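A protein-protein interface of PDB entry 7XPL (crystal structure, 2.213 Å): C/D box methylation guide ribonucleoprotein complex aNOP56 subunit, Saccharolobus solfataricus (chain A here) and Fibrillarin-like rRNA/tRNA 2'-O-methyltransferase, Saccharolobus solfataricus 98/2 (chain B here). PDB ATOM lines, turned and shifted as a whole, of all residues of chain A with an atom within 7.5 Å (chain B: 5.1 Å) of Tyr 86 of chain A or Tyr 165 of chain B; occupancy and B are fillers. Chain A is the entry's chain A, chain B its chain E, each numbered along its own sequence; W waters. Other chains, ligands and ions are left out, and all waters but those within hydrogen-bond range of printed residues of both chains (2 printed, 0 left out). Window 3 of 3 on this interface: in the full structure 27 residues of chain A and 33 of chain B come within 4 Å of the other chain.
Printed residues of chain B within 4 Å of Glu 66 of chain A: Gln 138 (3.5 Å). Of the printed residues of chain B, Tyr 83 of chain A touches Gln 138 (3.0 Å). Of chain B, only Tyr 165, Lys 168 and Phe 169 come within 4 Å of Tyr 86 of chain A. Printed residues of chain B within 4 Å of Arg 91 of chain A: Ala 167, Lys 168 and Phe 169. Ile 164 of chain B touches none of the printed residues of chain A. Tyr 165 of chain B touches just one residue of chain A: Tyr 86 (3.7 Å). Of the printed residues of chain A, Ala 167 of chain B touches Arg 91 (3.3 Å). Printed residues of chain A within 4 Å of Lys 168 of chain B: Tyr 86 (3.6 Å) and Arg 91 (2.9 Å). The nearest printed residue of chain B that does not touch Tyr 86 of chain A is Gln 138 of chain B (6.1 Å). The nearest residue of chain A that does not touch Tyr 165 of chain B is Tyr 83 of chain A (4.1 Å). The nearest printed residue of chain A that does not touch Phe 169 of chain B is Pro 85 of chain A (4.5 Å).
Hydrophobic or aromatic side chains of chain B within 4 Å of the printed part of chain A: Tyr 165 and Phe 169. Of the 12 printed residues of chain A, 5 touch a printed residue of chain B. Printed residues of chain A that touch a printed residue of chain B: Glu 66, Tyr 83, Tyr 86, Arg 91 and Arg 94. Hydrophobic or aromatic side chains of chain A that line the printed part of chain B: Tyr 83 and Tyr 86. Along chain A the printed residues that touch a printed residue of chain B span positions 66 to 94. Among the printed residues, 9 pairs touch across the chains.
Glu 66 of chain A touches Gln 138 of chain B (O to CG, 3.5 Å). Tyr 165 of chain B touches Tyr 86 of chain A (CE1 to CE2, 3.7 Å). Tyr 86 of chain A touches Lys 168 of chain B. Phe 169 of chain B touches Tyr 86 of chain A. Arg 91 of chain A touches Phe 169 of chain B.
The guanidinium group (NH1) of Arg 91 of chain A sits at hydrogen-bond distance from the backbone carbonyl oxygen (O) of Lys 168 of chain B. The guanidinium group of Arg 91 of chain A is in hydrogen-bond range of the backbone carbonyl oxygen of Ala 167 of chain B, at 3.3 Å. OH of Tyr 83 of chain A lies within hydrogen-bond range of NE2 of Gln 138 of chain B, at 3.0 Å. The guanidinium group of Arg 94 of chain A sits at hydrogen-bond distance from the backbone carbonyl oxygen of Phe 169 of chain B, at 2.7 Å.
Water W1 bridges OH of Tyr 165 of chain B (2.9 Å) and OH of Tyr 83 of chain A (3.1 Å). Water W2 lies within hydrogen-bond range of OH of Tyr 83 of chain A (3.0 Å) and NE2 of Gln 138 of chain B (3.5 Å).
OG of Ser 90 of chain A lies within hydrogen-bond range of NH1 of Arg 94 of chain A. The side-chain amide nitrogen (NE2) of Gln 138 of chain B lies within hydrogen-bond range of the side-chain hydroxyl (OH) of Tyr 165 of chain B (2.8 Å).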
ATOM      1  N   VAL A  65       7.664   3.073  -2.775  1.00  0.00           N
ATOM      2  CA  VAL A  65       6.230   3.119  -2.559  1.00  0.00           C
ATOM      3  C   VAL A  65       5.983   3.975  -1.334  1.00  0.00           C
ATOM      4  O   VAL A  65       6.888   4.230  -0.524  1.00  0.00           O
ATOM      5  CB  VAL A  65       5.585   1.730  -2.398  1.00  0.00           C
ATOM      6  CG1 VAL A  65       5.790   0.928  -3.660  1.00  0.00           C
ATOM      7  CG2 VAL A  65       6.139   1.001  -1.172  1.00  0.00           C
ATOM      8  N   GLU A  66       4.747   4.478  -1.245  1.00  0.00           N
ATOM      9  CA  GLU A  66       4.317   5.367  -0.167  1.00  0.00           C
ATOM     10  C   GLU A  66       3.681   4.618   0.991  1.00  0.00           C
ATOM     11  O   GLU A  66       3.663   5.140   2.109  1.00  0.00           O
ATOM     12  CB  GLU A  66       3.311   6.404  -0.692  1.00  0.00           C
ATOM     13  CG  GLU A  66       3.523   6.801  -2.163  1.00  0.00           C
ATOM     14  CD  GLU A  66       2.332   7.569  -2.770  1.00  0.00           C
ATOM     15  OE1 GLU A  66       2.178   8.779  -2.456  1.00  0.00           O
ATOM     16  OE2 GLU A  66       1.534   6.957  -3.543  1.00  0.00           O
ATOM     17  N   TYR A  83      10.300   1.382   0.762  1.00  0.00           N
ATOM     18  CA  TYR A  83       9.294   2.243   1.337  1.00  0.00           C
ATOM     19  C   TYR A  83       9.975   3.504   1.837  1.00  0.00           C
ATOM     20  O   TYR A  83      11.026   3.434   2.472  1.00  0.00           O
ATOM     21  CB  TYR A  83       8.570   1.538   2.484  1.00  0.00           C
ATOM     22  CG  TYR A  83       7.815   2.482   3.377  1.00  0.00           C
ATOM     23  CD1 TYR A  83       6.681   3.143   2.918  1.00  0.00           C
ATOM     24  CD2 TYR A  83       8.235   2.711   4.686  1.00  0.00           C
ATOM     25  CE1 TYR A  83       5.977   4.010   3.741  1.00  0.00           C
ATOM     26  CE2 TYR A  83       7.548   3.581   5.523  1.00  0.00           C
ATOM     27  CZ  TYR A  83       6.416   4.233   5.052  1.00  0.00           C
ATOM     28  OH  TYR A  83       5.719   5.110   5.885  1.00  0.00           O
ATOM     29  N   GLU A  84       9.379   4.653   1.541  1.00  0.00           N
ATOM     30  CA  GLU A  84       9.907   5.926   2.012  1.00  0.00           C
ATOM     31  C   GLU A  84       8.748   6.735   2.577  1.00  0.00           C
ATOM     32  O   GLU A  84       7.747   6.978   1.860  1.00  0.00           O
ATOM     33  CB  GLU A  84      10.621   6.690   0.902  1.00  0.00           C
ATOM     34  CG  GLU A  84      11.640   7.688   1.438  1.00  0.00           C
ATOM     35  CD  GLU A  84      12.155   8.647   0.369  1.00  0.00           C
ATOM     36  OE1 GLU A  84      12.114   9.883   0.594  1.00  0.00           O
ATOM     37  OE2 GLU A  84      12.593   8.165  -0.701  1.00  0.00           O
ATOM     38  N   PRO A  85       8.814   7.134   3.842  1.00  0.00           N
ATOM     39  CA  PRO A  85       7.790   8.019   4.392  1.00  0.00           C
ATOM     40  C   PRO A  85       7.896   9.417   3.798  1.00  0.00           C
ATOM     41  O   PRO A  85       8.994   9.898   3.496  1.00  0.00           O
ATOM     42  CB  PRO A  85       8.105   8.025   5.896  1.00  0.00           C
ATOM     43  CG  PRO A  85       9.551   7.729   5.977  1.00  0.00           C
ATOM     44  CD  PRO A  85       9.826   6.750   4.843  1.00  0.00           C
ATOM     45  N   TYR A  86       6.727  10.058   3.632  1.00  0.00           N
ATOM     46  CA  TYR A  86       6.585  11.436   3.160  1.00  0.00           C
ATOM     47  C   TYR A  86       7.718  11.899   2.241  1.00  0.00           C
ATOM     48  O   TYR A  86       8.350  12.931   2.503  1.00  0.00           O
ATOM     49  CB  TYR A  86       6.471  12.383   4.363  1.00  0.00           C
ATOM     50  CG  TYR A  86       7.466  12.075   5.464  1.00  0.00           C
ATOM     51  CD1 TYR A  86       8.822  12.327   5.295  1.00  0.00           C
ATOM     52  CD2 TYR A  86       7.059  11.521   6.664  1.00  0.00           C
ATOM     53  CE1 TYR A  86       9.739  12.039   6.286  1.00  0.00           C
ATOM     54  CE2 TYR A  86       7.979  11.235   7.668  1.00  0.00           C
ATOM     55  CZ  TYR A  86       9.316  11.498   7.468  1.00  0.00           C
ATOM     56  OH  TYR A  86      10.228  11.217   8.459  1.00  0.00           O
ATOM     57  N   SER A  87       7.967  11.164   1.155  1.00  0.00           N
ATOM     58  CA  SER A  87       9.073  11.481   0.260  1.00  0.00           C
ATOM     59  C   SER A  87       8.894  12.844  -0.401  1.00  0.00           C
ATOM     60  O   SER A  87       7.771  13.331  -0.596  1.00  0.00           O
ATOM     61  CB  SER A  87       9.205  10.420  -0.827  1.00  0.00           C
ATOM     62  OG  SER A  87       8.112  10.505  -1.723  1.00  0.00           O
ATOM     63  N   LYS A  88      10.036  13.446  -0.758  1.00  0.00           N
ATOM     64  CA  LYS A  88      10.052  14.714  -1.474  1.00  0.00           C
ATOM     65  C   LYS A  88       9.283  14.614  -2.777  1.00  0.00           C
ATOM     66  O   LYS A  88       8.529  15.521  -3.134  1.00  0.00           O
ATOM     67  CB  LYS A  88      11.500  15.140  -1.730  1.00  0.00           C
ATOM     68  CG  LYS A  88      11.779  15.784  -3.094  1.00  0.00           C
ATOM     69  CD  LYS A  88      13.290  15.860  -3.339  1.00  0.00           C
ATOM     70  CE  LYS A  88      13.636  16.116  -4.809  1.00  0.00           C
ATOM     71  NZ  LYS A  88      15.124  15.984  -5.067  1.00  0.00           N
ATOM     72  N   VAL A  89       9.436  13.505  -3.487  1.00  0.00           N
ATOM     73  CA  VAL A  89       8.771  13.375  -4.772  1.00  0.00           C
ATOM     74  C   VAL A  89       7.261  13.356  -4.594  1.00  0.00           C
ATOM     75  O   VAL A  89       6.531  13.935  -5.398  1.00  0.00           O
ATOM     76  CB  VAL A  89       9.267  12.118  -5.502  1.00  0.00           C
ATOM     77  CG1 VAL A  89       8.413  11.862  -6.735  1.00  0.00           C
ATOM     78  CG2 VAL A  89      10.745  12.270  -5.859  1.00  0.00           C
ATOM     79  N   SER A  90       6.764  12.681  -3.550  1.00  0.00           N
ATOM     80  CA  SER A  90       5.320  12.644  -3.346  1.00  0.00           C
ATOM     81  C   SER A  90       4.795  14.009  -2.908  1.00  0.00           C
ATOM     82  O   SER A  90       3.686  14.400  -3.297  1.00  0.00           O
ATOM     83  CB  SER A  90       4.948  11.545  -2.337  1.00  0.00           C
ATOM     84  OG  SER A  90       5.345  11.909  -1.029  1.00  0.00           O
ATOM     85  N   ARG A  91       5.596  14.771  -2.152  1.00  0.00           N
ATOM     86  CA  ARG A  91       5.231  16.161  -1.891  1.00  0.00           C
ATOM     87  C   ARG A  91       5.201  16.966  -3.182  1.00  0.00           C
ATOM     88  O   ARG A  91       4.326  17.814  -3.373  1.00  0.00           O
ATOM     89  CB  ARG A  91       6.186  16.793  -0.877  1.00  0.00           C
ATOM     90  CG  ARG A  91       5.975  16.257   0.533  1.00  0.00           C
ATOM     91  CD  ARG A  91       6.949  16.841   1.526  1.00  0.00           C
ATOM     92  NE  ARG A  91       6.897  18.299   1.522  1.00  0.00           N
ATOM     93  CZ  ARG A  91       6.142  19.053   2.318  1.00  0.00           C
ATOM     94  NH1 ARG A  91       5.326  18.510   3.219  1.00  0.00           N
ATOM     95  NH2 ARG A  91       6.200  20.372   2.210  1.00  0.00           N
ATOM     96  N   ARG A  94       1.918  16.243  -4.868  1.00  0.00           N
ATOM     97  CA  ARG A  94       0.701  16.788  -4.268  1.00  0.00           C
ATOM     98  C   ARG A  94       0.613  18.296  -4.454  1.00  0.00           C
ATOM     99  O   ARG A  94      -0.488  18.841  -4.586  1.00  0.00           O
ATOM    100  CB  ARG A  94       0.632  16.421  -2.788  1.00  0.00           C
ATOM    101  CG  ARG A  94       0.105  15.031  -2.560  1.00  0.00           C
ATOM    102  CD  ARG A  94      -0.119  14.763  -1.093  1.00  0.00           C
ATOM    103  NE  ARG A  94       1.114  14.767  -0.316  1.00  0.00           N
ATOM    104  CZ  ARG A  94       1.904  13.711  -0.180  1.00  0.00           C
ATOM    105  NH1 ARG A  94       2.998  13.804   0.561  1.00  0.00           N
ATOM    106  NH2 ARG A  94       1.588  12.563  -0.770  1.00  0.00           N
ATOM    107  N   ARG B 135      -2.975   9.011  12.714  1.00  0.00           N
ATOM    108  CA  ARG B 135      -1.671   8.369  12.843  1.00  0.00           C
ATOM    109  C   ARG B 135      -1.249   7.677  11.561  1.00  0.00           C
ATOM    110  O   ARG B 135      -0.097   7.246  11.458  1.00  0.00           O
ATOM    111  CB  ARG B 135      -1.675   7.360  14.008  1.00  0.00           C
ATOM    112  CG  ARG B 135      -1.640   8.034  15.391  1.00  0.00           C
ATOM    113  CD  ARG B 135      -1.802   7.059  16.589  1.00  0.00           C
ATOM    114  NE  ARG B 135      -2.977   6.211  16.405  1.00  0.00           N
ATOM    115  CZ  ARG B 135      -4.091   6.256  17.138  1.00  0.00           C
ATOM    116  NH1 ARG B 135      -4.187   7.095  18.164  1.00  0.00           N
ATOM    117  NH2 ARG B 135      -5.112   5.449  16.858  1.00  0.00           N
ATOM    118  N   PRO B 137      -1.286   8.700   7.942  1.00  0.00           N
ATOM    119  CA  PRO B 137      -1.482   9.568   6.768  1.00  0.00           C
ATOM    120  C   PRO B 137      -1.284   8.857   5.465  1.00  0.00           C
ATOM    121  O   PRO B 137      -1.716   9.383   4.438  1.00  0.00           O
ATOM    122  CB  PRO B 137      -0.448  10.679   6.951  1.00  0.00           C
ATOM    123  CG  PRO B 137       0.494  10.162   7.951  1.00  0.00           C
ATOM    124  CD  PRO B 137      -0.231   9.217   8.823  1.00  0.00           C
ATOM    125  N   GLN B 138      -0.662   7.675   5.469  1.00  0.00           N
ATOM    126  CA  GLN B 138      -0.570   6.874   4.254  1.00  0.00           C
ATOM    127  C   GLN B 138      -1.932   6.420   3.760  1.00  0.00           C
ATOM    128  O   GLN B 138      -2.054   6.009   2.602  1.00  0.00           O
ATOM    129  CB  GLN B 138       0.321   5.654   4.486  1.00  0.00           C
ATOM    130  CG  GLN B 138       1.741   6.020   4.874  1.00  0.00           C
ATOM    131  CD  GLN B 138       1.904   6.286   6.366  1.00  0.00           C
ATOM    132  OE1 GLN B 138       0.917   6.439   7.118  1.00  0.00           O
ATOM    133  NE2 GLN B 138       3.168   6.323   6.813  1.00  0.00           N
ATOM    134  N   THR B 160       0.877  16.114  19.343  1.00  0.00           N
ATOM    135  CA  THR B 160       1.854  17.006  18.728  1.00  0.00           C
ATOM    136  C   THR B 160       2.711  16.259  17.716  1.00  0.00           C
ATOM    137  O   THR B 160       2.954  16.755  16.609  1.00  0.00           O
ATOM    138  CB  THR B 160       2.725  17.651  19.799  1.00  0.00           C
ATOM    139  OG1 THR B 160       1.875  18.157  20.839  1.00  0.00           O
ATOM    140  CG2 THR B 160       3.526  18.818  19.192  1.00  0.00           C
ATOM    141  N   ASP B 161       3.131  15.040  18.063  1.00  0.00           N
ATOM    142  CA  ASP B 161       3.876  14.226  17.110  1.00  0.00           C
ATOM    143  C   ASP B 161       3.016  13.815  15.932  1.00  0.00           C
ATOM    144  O   ASP B 161       3.523  13.670  14.817  1.00  0.00           O
ATOM    145  CB  ASP B 161       4.429  13.000  17.806  1.00  0.00           C
ATOM    146  CG  ASP B 161       5.071  13.355  19.115  1.00  0.00           C
ATOM    147  OD1 ASP B 161       4.315  13.623  20.099  1.00  0.00           O
ATOM    148  OD2 ASP B 161       6.316  13.431  19.129  1.00  0.00           O
ATOM    149  N   ILE B 162       1.720  13.618  16.153  1.00  0.00           N
ATOM    150  CA  ILE B 162       0.849  13.314  15.030  1.00  0.00           C
ATOM    151  C   ILE B 162       0.719  14.533  14.125  1.00  0.00           C
ATOM    152  O   ILE B 162       0.697  14.408  12.897  1.00  0.00           O
ATOM    153  CB  ILE B 162      -0.523  12.825  15.524  1.00  0.00           C
ATOM    154  CG1 ILE B 162      -0.360  11.597  16.416  1.00  0.00           C
ATOM    155  CG2 ILE B 162      -1.405  12.500  14.327  1.00  0.00           C
ATOM    156  CD1 ILE B 162      -1.603  11.245  17.212  1.00  0.00           C
ATOM    157  N   ALA B 163       0.643  15.726  14.714  1.00  0.00           N
ATOM    158  CA  ALA B 163       0.592  16.946  13.914  1.00  0.00           C
ATOM    159  C   ALA B 163       1.874  17.114  13.107  1.00  0.00           C
ATOM    160  O   ALA B 163       1.838  17.386  11.901  1.00  0.00           O
ATOM    161  CB  ALA B 163       0.361  18.161  14.811  1.00  0.00           C
ATOM    162  N   ILE B 164       3.017  16.941  13.759  1.00  0.00           N
ATOM    163  CA  ILE B 164       4.295  17.087  13.068  1.00  0.00           C
ATOM    164  C   ILE B 164       4.403  16.085  11.923  1.00  0.00           C
ATOM    165  O   ILE B 164       4.806  16.437  10.805  1.00  0.00           O
ATOM    166  CB  ILE B 164       5.442  16.939  14.082  1.00  0.00           C
ATOM    167  CG1 ILE B 164       5.406  18.110  15.074  1.00  0.00           C
ATOM    168  CG2 ILE B 164       6.793  16.808  13.382  1.00  0.00           C
ATOM    169  CD1 ILE B 164       6.382  17.953  16.219  1.00  0.00           C
ATOM    170  N   TYR B 165       4.009  14.831  12.171  1.00  0.00           N
ATOM    171  CA  TYR B 165       4.113  13.783  11.157  1.00  0.00           C
ATOM    172  C   TYR B 165       3.183  14.050   9.966  1.00  0.00           C
ATOM    173  O   TYR B 165       3.573  13.854   8.808  1.00  0.00           O
ATOM    174  CB  TYR B 165       3.831  12.441  11.836  1.00  0.00           C
ATOM    175  CG  TYR B 165       4.007  11.167  11.046  1.00  0.00           C
ATOM    176  CD1 TYR B 165       5.200  10.853  10.428  1.00  0.00           C
ATOM    177  CD2 TYR B 165       2.988  10.219  11.008  1.00  0.00           C
ATOM    178  CE1 TYR B 165       5.360   9.641   9.743  1.00  0.00           C
ATOM    179  CE2 TYR B 165       3.130   9.010  10.323  1.00  0.00           C
ATOM    180  CZ  TYR B 165       4.317   8.722   9.692  1.00  0.00           C
ATOM    181  OH  TYR B 165       4.450   7.516   9.019  1.00  0.00           O
ATOM    182  N   ASN B 166       1.957  14.525  10.217  1.00  0.00           N
ATOM    183  CA  ASN B 166       1.090  14.908   9.102  1.00  0.00           C
ATOM    184  C   ASN B 166       1.658  16.110   8.346  1.00  0.00           C
ATOM    185  O   ASN B 166       1.518  16.200   7.124  1.00  0.00           O
ATOM    186  CB  ASN B 166      -0.333  15.201   9.609  1.00  0.00           C
ATOM    187  CG  ASN B 166      -1.189  13.937   9.728  1.00  0.00           C
ATOM    188  OD1 ASN B 166      -1.910  13.573   8.796  1.00  0.00           O
ATOM    189  ND2 ASN B 166      -1.079  13.246  10.857  1.00  0.00           N
ATOM    190  N   ALA B 167       2.321  17.025   9.055  1.00  0.00           N
ATOM    191  CA  ALA B 167       2.908  18.192   8.411  1.00  0.00           C
ATOM    192  C   ALA B 167       3.995  17.801   7.409  1.00  0.00           C
ATOM    193  O   ALA B 167       4.054  18.368   6.309  1.00  0.00           O
ATOM    194  CB  ALA B 167       3.466  19.147   9.467  1.00  0.00           C
ATOM    195  N   LYS B 168       4.841  16.814   7.748  1.00  0.00           N
ATOM    196  CA  LYS B 168       5.907  16.403   6.831  1.00  0.00           C
ATOM    197  C   LYS B 168       5.345  15.827   5.540  1.00  0.00           C
ATOM    198  O   LYS B 168       5.980  15.932   4.479  1.00  0.00           O
ATOM    199  CB  LYS B 168       6.833  15.386   7.504  1.00  0.00           C
ATOM    200  CG  LYS B 168       7.592  15.949   8.670  1.00  0.00           C
ATOM    201  CD  LYS B 168       8.454  14.870   9.327  1.00  0.00           C
ATOM    202  CE  LYS B 168       9.233  15.452  10.489  1.00  0.00           C
ATOM    203  NZ  LYS B 168      10.078  14.437  11.162  1.00  0.00           N
ATOM    204  N   PHE B 169       4.152  15.231   5.611  1.00  0.00           N
ATOM    205  CA  PHE B 169       3.476  14.726   4.420  1.00  0.00           C
ATOM    206  C   PHE B 169       2.860  15.846   3.582  1.00  0.00           C
ATOM    207  O   PHE B 169       2.971  15.842   2.352  1.00  0.00           O
ATOM    208  CB  PHE B 169       2.365  13.748   4.826  1.00  0.00           C
ATOM    209  CG  PHE B 169       2.814  12.320   4.960  1.00  0.00           C
ATOM    210  CD1 PHE B 169       3.226  11.828   6.183  1.00  0.00           C
ATOM    211  CD2 PHE B 169       2.804  11.473   3.863  1.00  0.00           C
ATOM    212  CE1 PHE B 169       3.633  10.527   6.310  1.00  0.00           C
ATOM    213  CE2 PHE B 169       3.206  10.170   3.981  1.00  0.00           C
ATOM    214  CZ  PHE B 169       3.620   9.694   5.214  1.00  0.00           C
HETATM  215  O   HOH W   1       6.820   5.824   8.728  1.00  0.00           O
HETATM  216  O   HOH W   2       3.491   3.181   5.347  1.00  0.00           O
